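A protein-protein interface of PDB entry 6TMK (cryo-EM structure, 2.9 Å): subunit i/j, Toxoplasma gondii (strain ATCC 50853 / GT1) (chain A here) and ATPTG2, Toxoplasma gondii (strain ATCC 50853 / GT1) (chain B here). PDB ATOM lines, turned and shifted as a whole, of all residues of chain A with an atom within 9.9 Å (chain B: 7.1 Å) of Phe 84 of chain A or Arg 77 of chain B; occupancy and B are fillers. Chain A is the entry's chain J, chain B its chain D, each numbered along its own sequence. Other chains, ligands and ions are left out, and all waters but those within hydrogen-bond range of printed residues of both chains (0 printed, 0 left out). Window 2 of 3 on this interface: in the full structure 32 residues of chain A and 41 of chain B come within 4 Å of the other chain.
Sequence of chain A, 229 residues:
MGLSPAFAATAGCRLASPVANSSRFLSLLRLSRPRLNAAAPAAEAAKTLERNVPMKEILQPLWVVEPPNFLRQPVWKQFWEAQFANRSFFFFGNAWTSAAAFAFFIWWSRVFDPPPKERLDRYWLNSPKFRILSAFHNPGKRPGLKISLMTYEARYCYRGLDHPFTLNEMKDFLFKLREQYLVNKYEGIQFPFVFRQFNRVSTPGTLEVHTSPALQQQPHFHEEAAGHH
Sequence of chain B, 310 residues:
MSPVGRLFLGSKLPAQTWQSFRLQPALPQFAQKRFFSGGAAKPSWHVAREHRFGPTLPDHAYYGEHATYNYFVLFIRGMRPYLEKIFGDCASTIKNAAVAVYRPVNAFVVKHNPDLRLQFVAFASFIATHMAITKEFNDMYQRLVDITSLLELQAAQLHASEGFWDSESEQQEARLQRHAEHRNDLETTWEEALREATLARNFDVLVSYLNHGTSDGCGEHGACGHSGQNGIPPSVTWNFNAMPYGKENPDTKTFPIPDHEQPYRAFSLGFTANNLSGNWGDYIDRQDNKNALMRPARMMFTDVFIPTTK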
ATOM      1  N   TRP A  76     -34.452  11.813  22.690  1.00  0.00           N
ATOM      2  CA  TRP A  76     -33.836  12.984  23.298  1.00  0.00           C
ATOM      3  C   TRP A  76     -32.327  12.842  23.379  1.00  0.00           C
ATOM      4  O   TRP A  76     -31.597  13.829  23.230  1.00  0.00           O
ATOM      5  CB  TRP A  76     -34.429  13.225  24.684  1.00  0.00           C
ATOM      6  CG  TRP A  76     -34.165  12.141  25.660  1.00  0.00           C
ATOM      7  CD1 TRP A  76     -34.964  11.079  25.939  1.00  0.00           C
ATOM      8  CD2 TRP A  76     -33.023  12.017  26.509  1.00  0.00           C
ATOM      9  NE1 TRP A  76     -34.389  10.296  26.903  1.00  0.00           N
ATOM     10  CE2 TRP A  76     -33.195  10.850  27.269  1.00  0.00           C
ATOM     11  CE3 TRP A  76     -31.870  12.778  26.695  1.00  0.00           C
ATOM     12  CZ2 TRP A  76     -32.258  10.427  28.198  1.00  0.00           C
ATOM     13  CZ3 TRP A  76     -30.945  12.354  27.614  1.00  0.00           C
ATOM     14  CH2 TRP A  76     -31.143  11.192  28.355  1.00  0.00           C
ATOM     15  N   LYS A  77     -31.836  11.617  23.547  1.00  0.00           N
ATOM     16  CA  LYS A  77     -30.398  11.402  23.584  1.00  0.00           C
ATOM     17  C   LYS A  77     -29.795  11.550  22.195  1.00  0.00           C
ATOM     18  O   LYS A  77     -28.686  12.080  22.042  1.00  0.00           O
ATOM     19  CB  LYS A  77     -30.111  10.028  24.179  1.00  0.00           C
ATOM     20  CG  LYS A  77     -28.691   9.813  24.602  1.00  0.00           C
ATOM     21  CD  LYS A  77     -28.500   8.426  25.163  1.00  0.00           C
ATOM     22  CE  LYS A  77     -28.960   8.345  26.602  1.00  0.00           C
ATOM     23  NZ  LYS A  77     -28.058   9.073  27.522  1.00  0.00           N
ATOM     24  N   GLN A  78     -30.513  11.094  21.169  1.00  0.00           N
ATOM     25  CA  GLN A  78     -30.091  11.361  19.798  1.00  0.00           C
ATOM     26  C   GLN A  78     -29.972  12.858  19.538  1.00  0.00           C
ATOM     27  O   GLN A  78     -28.980  13.326  18.967  1.00  0.00           O
ATOM     28  CB  GLN A  78     -31.071  10.736  18.815  1.00  0.00           C
ATOM     29  CG  GLN A  78     -31.184   9.244  18.898  1.00  0.00           C
ATOM     30  CD  GLN A  78     -32.181   8.687  17.920  1.00  0.00           C
ATOM     31  OE1 GLN A  78     -32.332   9.195  16.813  1.00  0.00           O
ATOM     32  NE2 GLN A  78     -32.869   7.632  18.318  1.00  0.00           N
ATOM     33  N   PHE A  79     -30.997  13.620  19.920  1.00  0.00           N
ATOM     34  CA  PHE A  79     -30.954  15.069  19.755  1.00  0.00           C
ATOM     35  C   PHE A  79     -29.756  15.671  20.484  1.00  0.00           C
ATOM     36  O   PHE A  79     -29.021  16.508  19.930  1.00  0.00           O
ATOM     37  CB  PHE A  79     -32.271  15.659  20.267  1.00  0.00           C
ATOM     38  CG  PHE A  79     -32.390  17.138  20.100  1.00  0.00           C
ATOM     39  CD1 PHE A  79     -32.811  17.672  18.904  1.00  0.00           C
ATOM     40  CD2 PHE A  79     -32.097  17.995  21.139  1.00  0.00           C
ATOM     41  CE1 PHE A  79     -32.924  19.022  18.740  1.00  0.00           C
ATOM     42  CE2 PHE A  79     -32.209  19.347  20.977  1.00  0.00           C
ATOM     43  CZ  PHE A  79     -32.624  19.864  19.778  1.00  0.00           C
ATOM     44  N   TRP A  80     -29.509  15.209  21.708  1.00  0.00           N
ATOM     45  CA  TRP A  80     -28.411  15.737  22.504  1.00  0.00           C
ATOM     46  C   TRP A  80     -27.074  15.495  21.817  1.00  0.00           C
ATOM     47  O   TRP A  80     -26.231  16.394  21.737  1.00  0.00           O
ATOM     48  CB  TRP A  80     -28.435  15.094  23.885  1.00  0.00           C
ATOM     49  CG  TRP A  80     -27.470  15.674  24.849  1.00  0.00           C
ATOM     50  CD1 TRP A  80     -26.455  15.026  25.471  1.00  0.00           C
ATOM     51  CD2 TRP A  80     -27.441  17.019  25.325  1.00  0.00           C
ATOM     52  NE1 TRP A  80     -25.783  15.882  26.299  1.00  0.00           N
ATOM     53  CE2 TRP A  80     -26.370  17.115  26.228  1.00  0.00           C
ATOM     54  CE3 TRP A  80     -28.211  18.154  25.073  1.00  0.00           C
ATOM     55  CZ2 TRP A  80     -26.052  18.296  26.879  1.00  0.00           C
ATOM     56  CZ3 TRP A  80     -27.890  19.324  25.717  1.00  0.00           C
ATOM     57  CH2 TRP A  80     -26.821  19.387  26.611  1.00  0.00           C
ATOM     58  N   GLU A  81     -26.861  14.279  21.317  1.00  0.00           N
ATOM     59  CA  GLU A  81     -25.601  13.971  20.650  1.00  0.00           C
ATOM     60  C   GLU A  81     -25.464  14.741  19.344  1.00  0.00           C
ATOM     61  O   GLU A  81     -24.350  15.121  18.948  1.00  0.00           O
ATOM     62  CB  GLU A  81     -25.507  12.471  20.416  1.00  0.00           C
ATOM     63  CG  GLU A  81     -24.114  11.975  20.173  1.00  0.00           C
ATOM     64  CD  GLU A  81     -23.279  11.944  21.436  1.00  0.00           C
ATOM     65  OE1 GLU A  81     -22.147  12.473  21.417  1.00  0.00           O
ATOM     66  OE2 GLU A  81     -23.760  11.401  22.453  1.00  0.00           O
ATOM     67  N   ALA A  82     -26.581  14.972  18.658  1.00  0.00           N
ATOM     68  CA  ALA A  82     -26.540  15.738  17.426  1.00  0.00           C
ATOM     69  C   ALA A  82     -26.060  17.152  17.692  1.00  0.00           C
ATOM     70  O   ALA A  82     -25.414  17.761  16.833  1.00  0.00           O
ATOM     71  CB  ALA A  82     -27.910  15.750  16.767  1.00  0.00           C
ATOM     72  N   GLN A  83     -26.372  17.696  18.869  1.00  0.00           N
ATOM     73  CA  GLN A  83     -25.968  19.075  19.136  1.00  0.00           C
ATOM     74  C   GLN A  83     -24.453  19.228  19.137  1.00  0.00           C
ATOM     75  O   GLN A  83     -23.938  20.283  18.751  1.00  0.00           O
ATOM     76  CB  GLN A  83     -26.547  19.566  20.457  1.00  0.00           C
ATOM     77  CG  GLN A  83     -28.031  19.443  20.543  1.00  0.00           C
ATOM     78  CD  GLN A  83     -28.714  20.136  19.398  1.00  0.00           C
ATOM     79  OE1 GLN A  83     -28.619  21.352  19.248  1.00  0.00           O
ATOM     80  NE2 GLN A  83     -29.379  19.364  18.561  1.00  0.00           N
ATOM     81  N   PHE A  84     -23.725  18.203  19.563  1.00  0.00           N
ATOM     82  CA  PHE A  84     -22.273  18.270  19.589  1.00  0.00           C
ATOM     83  C   PHE A  84     -21.646  17.710  18.328  1.00  0.00           C
ATOM     84  O   PHE A  84     -20.464  17.962  18.075  1.00  0.00           O
ATOM     85  CB  PHE A  84     -21.737  17.537  20.814  1.00  0.00           C
ATOM     86  CG  PHE A  84     -22.419  17.920  22.077  1.00  0.00           C
ATOM     87  CD1 PHE A  84     -23.445  17.162  22.587  1.00  0.00           C
ATOM     88  CD2 PHE A  84     -22.030  19.050  22.756  1.00  0.00           C
ATOM     89  CE1 PHE A  84     -24.065  17.530  23.747  1.00  0.00           C
ATOM     90  CE2 PHE A  84     -22.650  19.416  23.913  1.00  0.00           C
ATOM     91  CZ  PHE A  84     -23.664  18.656  24.411  1.00  0.00           C
ATOM     92  N   ALA A  85     -22.399  16.949  17.544  1.00  0.00           N
ATOM     93  CA  ALA A  85     -21.954  16.642  16.194  1.00  0.00           C
ATOM     94  C   ALA A  85     -21.862  17.925  15.366  1.00  0.00           C
ATOM     95  O   ALA A  85     -22.457  18.954  15.693  1.00  0.00           O
ATOM     96  CB  ALA A  85     -22.892  15.647  15.524  1.00  0.00           C
ATOM     97  N   ASN A  86     -21.102  17.852  14.280  1.00  0.00           N
ATOM     98  CA  ASN A  86     -20.830  19.021  13.456  1.00  0.00           C
ATOM     99  C   ASN A  86     -21.956  19.274  12.458  1.00  0.00           C
ATOM    100  O   ASN A  86     -22.548  18.339  11.912  1.00  0.00           O
ATOM    101  CB  ASN A  86     -19.505  18.842  12.722  1.00  0.00           C
ATOM    102  CG  ASN A  86     -19.004  20.120  12.107  1.00  0.00           C
ATOM    103  OD1 ASN A  86     -19.228  21.209  12.630  1.00  0.00           O
ATOM    104  ND2 ASN A  86     -18.316  19.996  10.989  1.00  0.00           N
ATOM    105  N   ARG A  87     -22.233  20.557  12.211  1.00  0.00           N
ATOM    106  CA  ARG A  87     -23.310  20.997  11.323  1.00  0.00           C
ATOM    107  C   ARG A  87     -24.668  20.492  11.789  1.00  0.00           C
ATOM    108  O   ARG A  87     -25.582  20.297  10.988  1.00  0.00           O
ATOM    109  CB  ARG A  87     -23.071  20.572   9.875  1.00  0.00           C
ATOM    110  CG  ARG A  87     -21.736  20.958   9.315  1.00  0.00           C
ATOM    111  CD  ARG A  87     -21.444  20.154   8.076  1.00  0.00           C
ATOM    112  NE  ARG A  87     -22.588  20.149   7.170  1.00  0.00           N
ATOM    113  CZ  ARG A  87     -22.902  19.149   6.352  1.00  0.00           C
ATOM    114  NH1 ARG A  87     -22.154  18.058   6.298  1.00  0.00           N
ATOM    115  NH2 ARG A  87     -23.968  19.246   5.574  1.00  0.00           N
ATOM    116  N   SER A  88     -24.804  20.289  13.095  1.00  0.00           N
ATOM    117  CA  SER A  88     -26.023  19.733  13.664  1.00  0.00           C
ATOM    118  C   SER A  88     -26.454  20.497  14.909  1.00  0.00           C
ATOM    119  O   SER A  88     -27.242  19.976  15.705  1.00  0.00           O
ATOM    120  CB  SER A  88     -25.832  18.260  13.997  1.00  0.00           C
ATOM    121  OG  SER A  88     -25.793  17.475  12.830  1.00  0.00           O
ATOM    122  N   PHE A  89     -25.966  21.720  15.090  1.00  0.00           N
ATOM    123  CA  PHE A  89     -26.370  22.533  16.223  1.00  0.00           C
ATOM    124  C   PHE A  89     -27.817  22.991  16.030  1.00  0.00           C
ATOM    125  O   PHE A  89     -28.471  22.674  15.035  1.00  0.00           O
ATOM    126  CB  PHE A  89     -25.404  23.699  16.413  1.00  0.00           C
ATOM    127  CG  PHE A  89     -25.491  24.337  17.765  1.00  0.00           C
ATOM    128  CD1 PHE A  89     -25.301  23.585  18.905  1.00  0.00           C
ATOM    129  CD2 PHE A  89     -25.796  25.673  17.901  1.00  0.00           C
ATOM    130  CE1 PHE A  89     -25.396  24.153  20.143  1.00  0.00           C
ATOM    131  CE2 PHE A  89     -25.894  26.243  19.144  1.00  0.00           C
ATOM    132  CZ  PHE A  89     -25.693  25.480  20.265  1.00  0.00           C
ATOM    133  N   PHE A  90     -28.310  23.772  16.988  1.00  0.00           N
ATOM    134  CA  PHE A  90     -29.705  23.750  17.396  1.00  0.00           C
ATOM    135  C   PHE A  90     -30.642  23.717  16.196  1.00  0.00           C
ATOM    136  O   PHE A  90     -31.230  22.668  15.920  1.00  0.00           O
ATOM    137  CB  PHE A  90     -29.956  24.974  18.279  1.00  0.00           C
ATOM    138  CG  PHE A  90     -31.360  25.116  18.770  1.00  0.00           C
ATOM    139  CD1 PHE A  90     -31.928  24.154  19.582  1.00  0.00           C
ATOM    140  CD2 PHE A  90     -32.090  26.242  18.470  1.00  0.00           C
ATOM    141  CE1 PHE A  90     -33.209  24.303  20.050  1.00  0.00           C
ATOM    142  CE2 PHE A  90     -33.372  26.396  18.935  1.00  0.00           C
ATOM    143  CZ  PHE A  90     -33.933  25.425  19.726  1.00  0.00           C
ATOM    144  N   THR A  97     -32.973  16.907  13.621  1.00  0.00           N
ATOM    145  CA  THR A  97     -32.784  17.676  14.840  1.00  0.00           C
ATOM    146  C   THR A  97     -32.878  19.161  14.546  1.00  0.00           C
ATOM    147  O   THR A  97     -33.469  19.923  15.319  1.00  0.00           O
ATOM    148  CB  THR A  97     -31.438  17.334  15.466  1.00  0.00           C
ATOM    149  OG1 THR A  97     -30.395  17.576  14.518  1.00  0.00           O
ATOM    150  CG2 THR A  97     -31.413  15.893  15.877  1.00  0.00           C
ATOM    151  N   THR B  68     -14.178  20.928   9.685  1.00  0.00           N
ATOM    152  CA  THR B  68     -14.688  19.906  10.584  1.00  0.00           C
ATOM    153  C   THR B  68     -14.218  20.059  12.020  1.00  0.00           C
ATOM    154  O   THR B  68     -14.922  19.624  12.931  1.00  0.00           O
ATOM    155  CB  THR B  68     -14.301  18.513  10.071  1.00  0.00           C
ATOM    156  OG1 THR B  68     -14.685  17.516  11.021  1.00  0.00           O
ATOM    157  CG2 THR B  68     -12.842  18.422   9.819  1.00  0.00           C
ATOM    158  N   TYR B  69     -13.052  20.656  12.247  1.00  0.00           N
ATOM    159  CA  TYR B  69     -12.564  20.956  13.589  1.00  0.00           C
ATOM    160  C   TYR B  69     -12.504  22.472  13.715  1.00  0.00           C
ATOM    161  O   TYR B  69     -11.446  23.085  13.583  1.00  0.00           O
ATOM    162  CB  TYR B  69     -11.215  20.325  13.854  1.00  0.00           C
ATOM    163  CG  TYR B  69     -11.189  18.839  13.659  1.00  0.00           C
ATOM    164  CD1 TYR B  69     -12.039  18.018  14.369  1.00  0.00           C
ATOM    165  CD2 TYR B  69     -10.312  18.256  12.767  1.00  0.00           C
ATOM    166  CE1 TYR B  69     -12.023  16.665  14.191  1.00  0.00           C
ATOM    167  CE2 TYR B  69     -10.289  16.903  12.586  1.00  0.00           C
ATOM    168  CZ  TYR B  69     -11.148  16.109  13.298  1.00  0.00           C
ATOM    169  OH  TYR B  69     -11.129  14.750  13.117  1.00  0.00           O
ATOM    170  N   ASN B  70     -13.646  23.069  14.005  1.00  0.00           N
ATOM    171  CA  ASN B  70     -13.766  24.512  14.054  1.00  0.00           C
ATOM    172  C   ASN B  70     -13.957  24.988  15.488  1.00  0.00           C
ATOM    173  O   ASN B  70     -14.118  24.205  16.437  1.00  0.00           O
ATOM    174  CB  ASN B  70     -14.899  24.985  13.146  1.00  0.00           C
ATOM    175  CG  ASN B  70     -16.235  24.408  13.526  1.00  0.00           C
ATOM    176  OD1 ASN B  70     -16.775  24.693  14.590  1.00  0.00           O
ATOM    177  ND2 ASN B  70     -16.785  23.598  12.646  1.00  0.00           N
ATOM    178  N   TYR B  71     -13.972  26.311  15.621  1.00  0.00           N
ATOM    179  CA  TYR B  71     -13.914  26.935  16.932  1.00  0.00           C
ATOM    180  C   TYR B  71     -15.145  26.583  17.748  1.00  0.00           C
ATOM    181  O   TYR B  71     -15.041  26.178  18.912  1.00  0.00           O
ATOM    182  CB  TYR B  71     -13.796  28.447  16.773  1.00  0.00           C
ATOM    183  CG  TYR B  71     -12.765  28.897  15.773  1.00  0.00           C
ATOM    184  CD1 TYR B  71     -11.470  28.419  15.811  1.00  0.00           C
ATOM    185  CD2 TYR B  71     -13.095  29.801  14.783  1.00  0.00           C
ATOM    186  CE1 TYR B  71     -10.536  28.835  14.892  1.00  0.00           C
ATOM    187  CE2 TYR B  71     -12.171  30.219  13.866  1.00  0.00           C
ATOM    188  CZ  TYR B  71     -10.895  29.737  13.923  1.00  0.00           C
ATOM    189  OH  TYR B  71      -9.981  30.161  12.994  1.00  0.00           O
ATOM    190  N   PHE B  72     -16.323  26.711  17.143  1.00  0.00           N
ATOM    191  CA  PHE B  72     -17.548  26.490  17.891  1.00  0.00           C
ATOM    192  C   PHE B  72     -17.701  25.036  18.295  1.00  0.00           C
ATOM    193  O   PHE B  72     -18.161  24.742  19.401  1.00  0.00           O
ATOM    194  CB  PHE B  72     -18.765  26.914  17.087  1.00  0.00           C
ATOM    195  CG  PHE B  72     -20.044  26.592  17.771  1.00  0.00           C
ATOM    196  CD1 PHE B  72     -20.491  27.371  18.813  1.00  0.00           C
ATOM    197  CD2 PHE B  72     -20.774  25.480  17.415  1.00  0.00           C
ATOM    198  CE1 PHE B  72     -21.647  27.067  19.461  1.00  0.00           C
ATOM    199  CE2 PHE B  72     -21.930  25.175  18.061  1.00  0.00           C
ATOM    200  CZ  PHE B  72     -22.368  25.970  19.090  1.00  0.00           C
ATOM    201  N   VAL B  73     -17.370  24.109  17.402  1.00  0.00           N
ATOM    202  CA  VAL B  73     -17.595  22.710  17.724  1.00  0.00           C
ATOM    203  C   VAL B  73     -16.624  22.263  18.806  1.00  0.00           C
ATOM    204  O   VAL B  73     -17.003  21.533  19.730  1.00  0.00           O
ATOM    205  CB  VAL B  73     -17.501  21.840  16.458  1.00  0.00           C
ATOM    206  CG1 VAL B  73     -16.078  21.628  16.041  1.00  0.00           C
ATOM    207  CG2 VAL B  73     -18.217  20.534  16.651  1.00  0.00           C
ATOM    208  N   LEU B  74     -15.378  22.743  18.756  1.00  0.00           N
ATOM    209  CA  LEU B  74     -14.460  22.456  19.853  1.00  0.00           C
ATOM    210  C   LEU B  74     -14.949  23.075  21.159  1.00  0.00           C
ATOM    211  O   LEU B  74     -14.888  22.444  22.222  1.00  0.00           O
ATOM    212  CB  LEU B  74     -13.067  22.962  19.504  1.00  0.00           C
ATOM    213  CG  LEU B  74     -12.379  22.302  18.311  1.00  0.00           C
ATOM    214  CD1 LEU B  74     -11.086  22.988  17.991  1.00  0.00           C
ATOM    215  CD2 LEU B  74     -12.133  20.842  18.549  1.00  0.00           C
ATOM    216  N   PHE B  75     -15.468  24.300  21.094  1.00  0.00           N
ATOM    217  CA  PHE B  75     -15.967  24.976  22.284  1.00  0.00           C
ATOM    218  C   PHE B  75     -17.117  24.208  22.923  1.00  0.00           C
ATOM    219  O   PHE B  75     -17.123  23.958  24.134  1.00  0.00           O
ATOM    220  CB  PHE B  75     -16.386  26.398  21.917  1.00  0.00           C
ATOM    221  CG  PHE B  75     -16.994  27.163  23.043  1.00  0.00           C
ATOM    222  CD1 PHE B  75     -16.218  27.621  24.084  1.00  0.00           C
ATOM    223  CD2 PHE B  75     -18.343  27.437  23.054  1.00  0.00           C
ATOM    224  CE1 PHE B  75     -16.776  28.321  25.115  1.00  0.00           C
ATOM    225  CE2 PHE B  75     -18.905  28.136  24.085  1.00  0.00           C
ATOM    226  CZ  PHE B  75     -18.121  28.582  25.117  1.00  0.00           C
ATOM    227  N   ILE B  76     -18.118  23.843  22.122  1.00  0.00           N
ATOM    228  CA  ILE B  76     -19.288  23.167  22.661  1.00  0.00           C
ATOM    229  C   ILE B  76     -18.928  21.766  23.136  1.00  0.00           C
ATOM    230  O   ILE B  76     -19.490  21.276  24.124  1.00  0.00           O
ATOM    231  CB  ILE B  76     -20.402  23.156  21.599  1.00  0.00           C
ATOM    232  CG1 ILE B  76     -21.758  22.865  22.224  1.00  0.00           C
ATOM    233  CG2 ILE B  76     -20.117  22.149  20.523  1.00  0.00           C
ATOM    234  CD1 ILE B  76     -22.319  24.028  22.963  1.00  0.00           C
ATOM    235  N   ARG B  77     -17.976  21.105  22.476  1.00  0.00           N
ATOM    236  CA  ARG B  77     -17.499  19.826  22.981  1.00  0.00           C
ATOM    237  C   ARG B  77     -16.798  19.983  24.321  1.00  0.00           C
ATOM    238  O   ARG B  77     -16.842  19.070  25.153  1.00  0.00           O
ATOM    239  CB  ARG B  77     -16.587  19.172  21.955  1.00  0.00           C
ATOM    240  CG  ARG B  77     -17.350  18.620  20.787  1.00  0.00           C
ATOM    241  CD  ARG B  77     -16.472  18.086  19.702  1.00  0.00           C
ATOM    242  NE  ARG B  77     -17.235  17.829  18.493  1.00  0.00           N
ATOM    243  CZ  ARG B  77     -16.723  17.359  17.366  1.00  0.00           C
ATOM    244  NH1 ARG B  77     -15.442  17.075  17.283  1.00  0.00           N
ATOM    245  NH2 ARG B  77     -17.503  17.156  16.323  1.00  0.00           N
ATOM    246  N   GLY B  78     -16.143  21.121  24.549  1.00  0.00           N
ATOM    247  CA  GLY B  78     -15.555  21.367  25.852  1.00  0.00           C
ATOM    248  C   GLY B  78     -16.585  21.680  26.915  1.00  0.00           C
ATOM    249  O   GLY B  78     -16.408  21.317  28.081  1.00  0.00           O
ATOM    250  N   MET B  79     -17.663  22.362  26.539  1.00  0.00           N
ATOM    251  CA  MET B  79     -18.711  22.729  27.484  1.00  0.00           C
ATOM    252  C   MET B  79     -19.735  21.625  27.704  1.00  0.00           C
ATOM    253  O   MET B  79     -20.616  21.785  28.553  1.00  0.00           O
ATOM    254  CB  MET B  79     -19.446  23.984  27.012  1.00  0.00           C
ATOM    255  CG  MET B  79     -18.599  25.226  26.920  1.00  0.00           C
ATOM    256  SD  MET B  79     -17.648  25.554  28.412  1.00  0.00           S
ATOM    257  CE  MET B  79     -15.989  25.445  27.769  1.00  0.00           C
ATOM    258  N   ARG B  80     -19.646  20.527  26.965  1.00  0.00           N
ATOM    259  CA  ARG B  80     -20.585  19.425  27.152  1.00  0.00           C
ATOM    260  C   ARG B  80     -20.750  18.968  28.595  1.00  0.00           C
ATOM    261  O   ARG B  80     -21.900  18.740  29.008  1.00  0.00           O
ATOM    262  CB  ARG B  80     -20.148  18.248  26.275  1.00  0.00           C
ATOM    263  CG  ARG B  80     -20.962  17.012  26.491  1.00  0.00           C
ATOM    264  CD  ARG B  80     -20.824  16.055  25.351  1.00  0.00           C
ATOM    265  NE  ARG B  80     -21.867  15.044  25.381  1.00  0.00           N
ATOM    266  CZ  ARG B  80     -22.096  14.181  24.402  1.00  0.00           C
ATOM    267  NH1 ARG B  80     -21.354  14.201  23.311  1.00  0.00           N
ATOM    268  NH2 ARG B  80     -23.071  13.300  24.518  1.00  0.00           N
ATOM    269  N   PRO B  81     -19.698  18.791  29.397  1.00  0.00           N
ATOM    270  CA  PRO B  81     -19.919  18.274  30.756  1.00  0.00           C
ATOM    271  C   PRO B  81     -20.730  19.209  31.636  1.00  0.00           C
ATOM    272  O   PRO B  81     -21.622  18.758  32.368  1.00  0.00           O
ATOM    273  CB  PRO B  81     -18.492  18.085  31.288  1.00  0.00           C
ATOM    274  CG  PRO B  81     -17.639  18.056  30.089  1.00  0.00           C
ATOM    275  CD  PRO B  81     -18.268  18.974  29.125  1.00  0.00           C
ATOM    276  N   LEU B  83     -22.899  21.500  30.692  1.00  0.00           N
ATOM    277  CA  LEU B  83     -24.274  21.511  30.215  1.00  0.00           C
ATOM    278  C   LEU B  83     -25.010  20.247  30.624  1.00  0.00           C
ATOM    279  O   LEU B  83     -26.197  20.292  30.967  1.00  0.00           O
ATOM    280  CB  LEU B  83     -24.289  21.666  28.702  1.00  0.00           C
ATOM    281  CG  LEU B  83     -23.829  23.013  28.174  1.00  0.00           C
ATOM    282  CD1 LEU B  83     -23.518  22.895  26.712  1.00  0.00           C
ATOM    283  CD2 LEU B  83     -24.890  24.058  28.419  1.00  0.00           C
ATOM    284  N   GLU B  84     -24.328  19.104  30.572  1.00  0.00           N
ATOM    285  CA  GLU B  84     -24.943  17.865  31.024  1.00  0.00           C
ATOM    286  C   GLU B  84     -25.322  17.958  32.492  1.00  0.00           C
ATOM    287  O   GLU B  84     -26.443  17.614  32.878  1.00  0.00           O
ATOM    288  CB  GLU B  84     -23.996  16.695  30.781  1.00  0.00           C
ATOM    289  CG  GLU B  84     -24.024  16.179  29.361  1.00  0.00           C
ATOM    290  CD  GLU B  84     -23.049  15.051  29.118  1.00  0.00           C
ATOM    291  OE1 GLU B  84     -22.035  14.967  29.842  1.00  0.00           O
ATOM    292  OE2 GLU B  84     -23.298  14.246  28.199  1.00  0.00           O
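Among the printed residues, 11 pairs touch across the chains.
Among the printed residues, Asp or Glu carboxylates within 4 Å of a Lys or Arg side-chain nitrogen of the other chain: Glu 81 of chain A with Arg 80 of chain B (2.7 Å).
OD1 of Asn 86 of chain A lies within hydrogen-bond range of ND2 of Asn 70 of chain B, 3.4 Å away.
The guanidinium group of Arg 80 of chain B is in salt-bridge range of the side-chain carboxylate of Glu 81 of chain A.
The guanidinium group of Arg 77 of chain B sits at hydrogen-bond distance from the backbone carbonyl oxygen of Phe 84 of chain A (3.3 Å).
Phe 84 of chain A touches just these residues of chain B: Val 73, Ile 76, Arg 77 and Arg 80.
Of the printed residues of chain A, Asn 70 of chain B touches Asn 86 (3.4 Å).
Printed residues of chain A within 4 Å of Phe 72 of chain B: Phe 89 (3.5 Å).
Printed residues of chain A within 4 Å of Val 73 of chain B: Phe 84 (3.7 Å).
Ile 76 of chain B touches one residue of chain A.
No residue of chain A comes within 4 Å of Gly 78 of chain B.
Printed residues of chain A within 4 Å of Arg 80 of chain B: Trp 80 (3.9 Å), Glu 81 (2.7 Å) and Phe 84 (3.6 Å).
The nearest residue of chain B that does not touch Phe 84 of chain A is Leu 83 of chain B (4.5 Å).
N of Val 73 of chain B is in hydrogen-bond range of OD1 of Asn 70 of chain B, at 2.9 Å.
O of Asn 86 of chain A sits at hydrogen-bond distance from OG of Ser 88 of chain A, 3.5 Å away.
The guanidinium group of Arg 80 of chain B lies within salt-bridge range of the side-chain carboxylate of Glu 84 of chain B (3.3 Å).
OD1 of Asn 70 of chain B lies within hydrogen-bond range of N of Phe 72 of chain B (3.3 Å).
Among the printed residues, merely in contact across the chains: Trp 80 of chain A with Arg 80 of chain B, Trp 80 of chain A with Leu 83 of chain B, Trp 80 of chain A with Glu 84 of chain B, Phe 84 of chain A with Val 73 of chain B, Phe 84 of chain A with Ile 76 of chain B, Phe 84 of chain A with Arg 80 of chain B, Asn 86 of chain A with Thr 68 of chain B and Phe 89 of chain A with Phe 72 of chain B.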
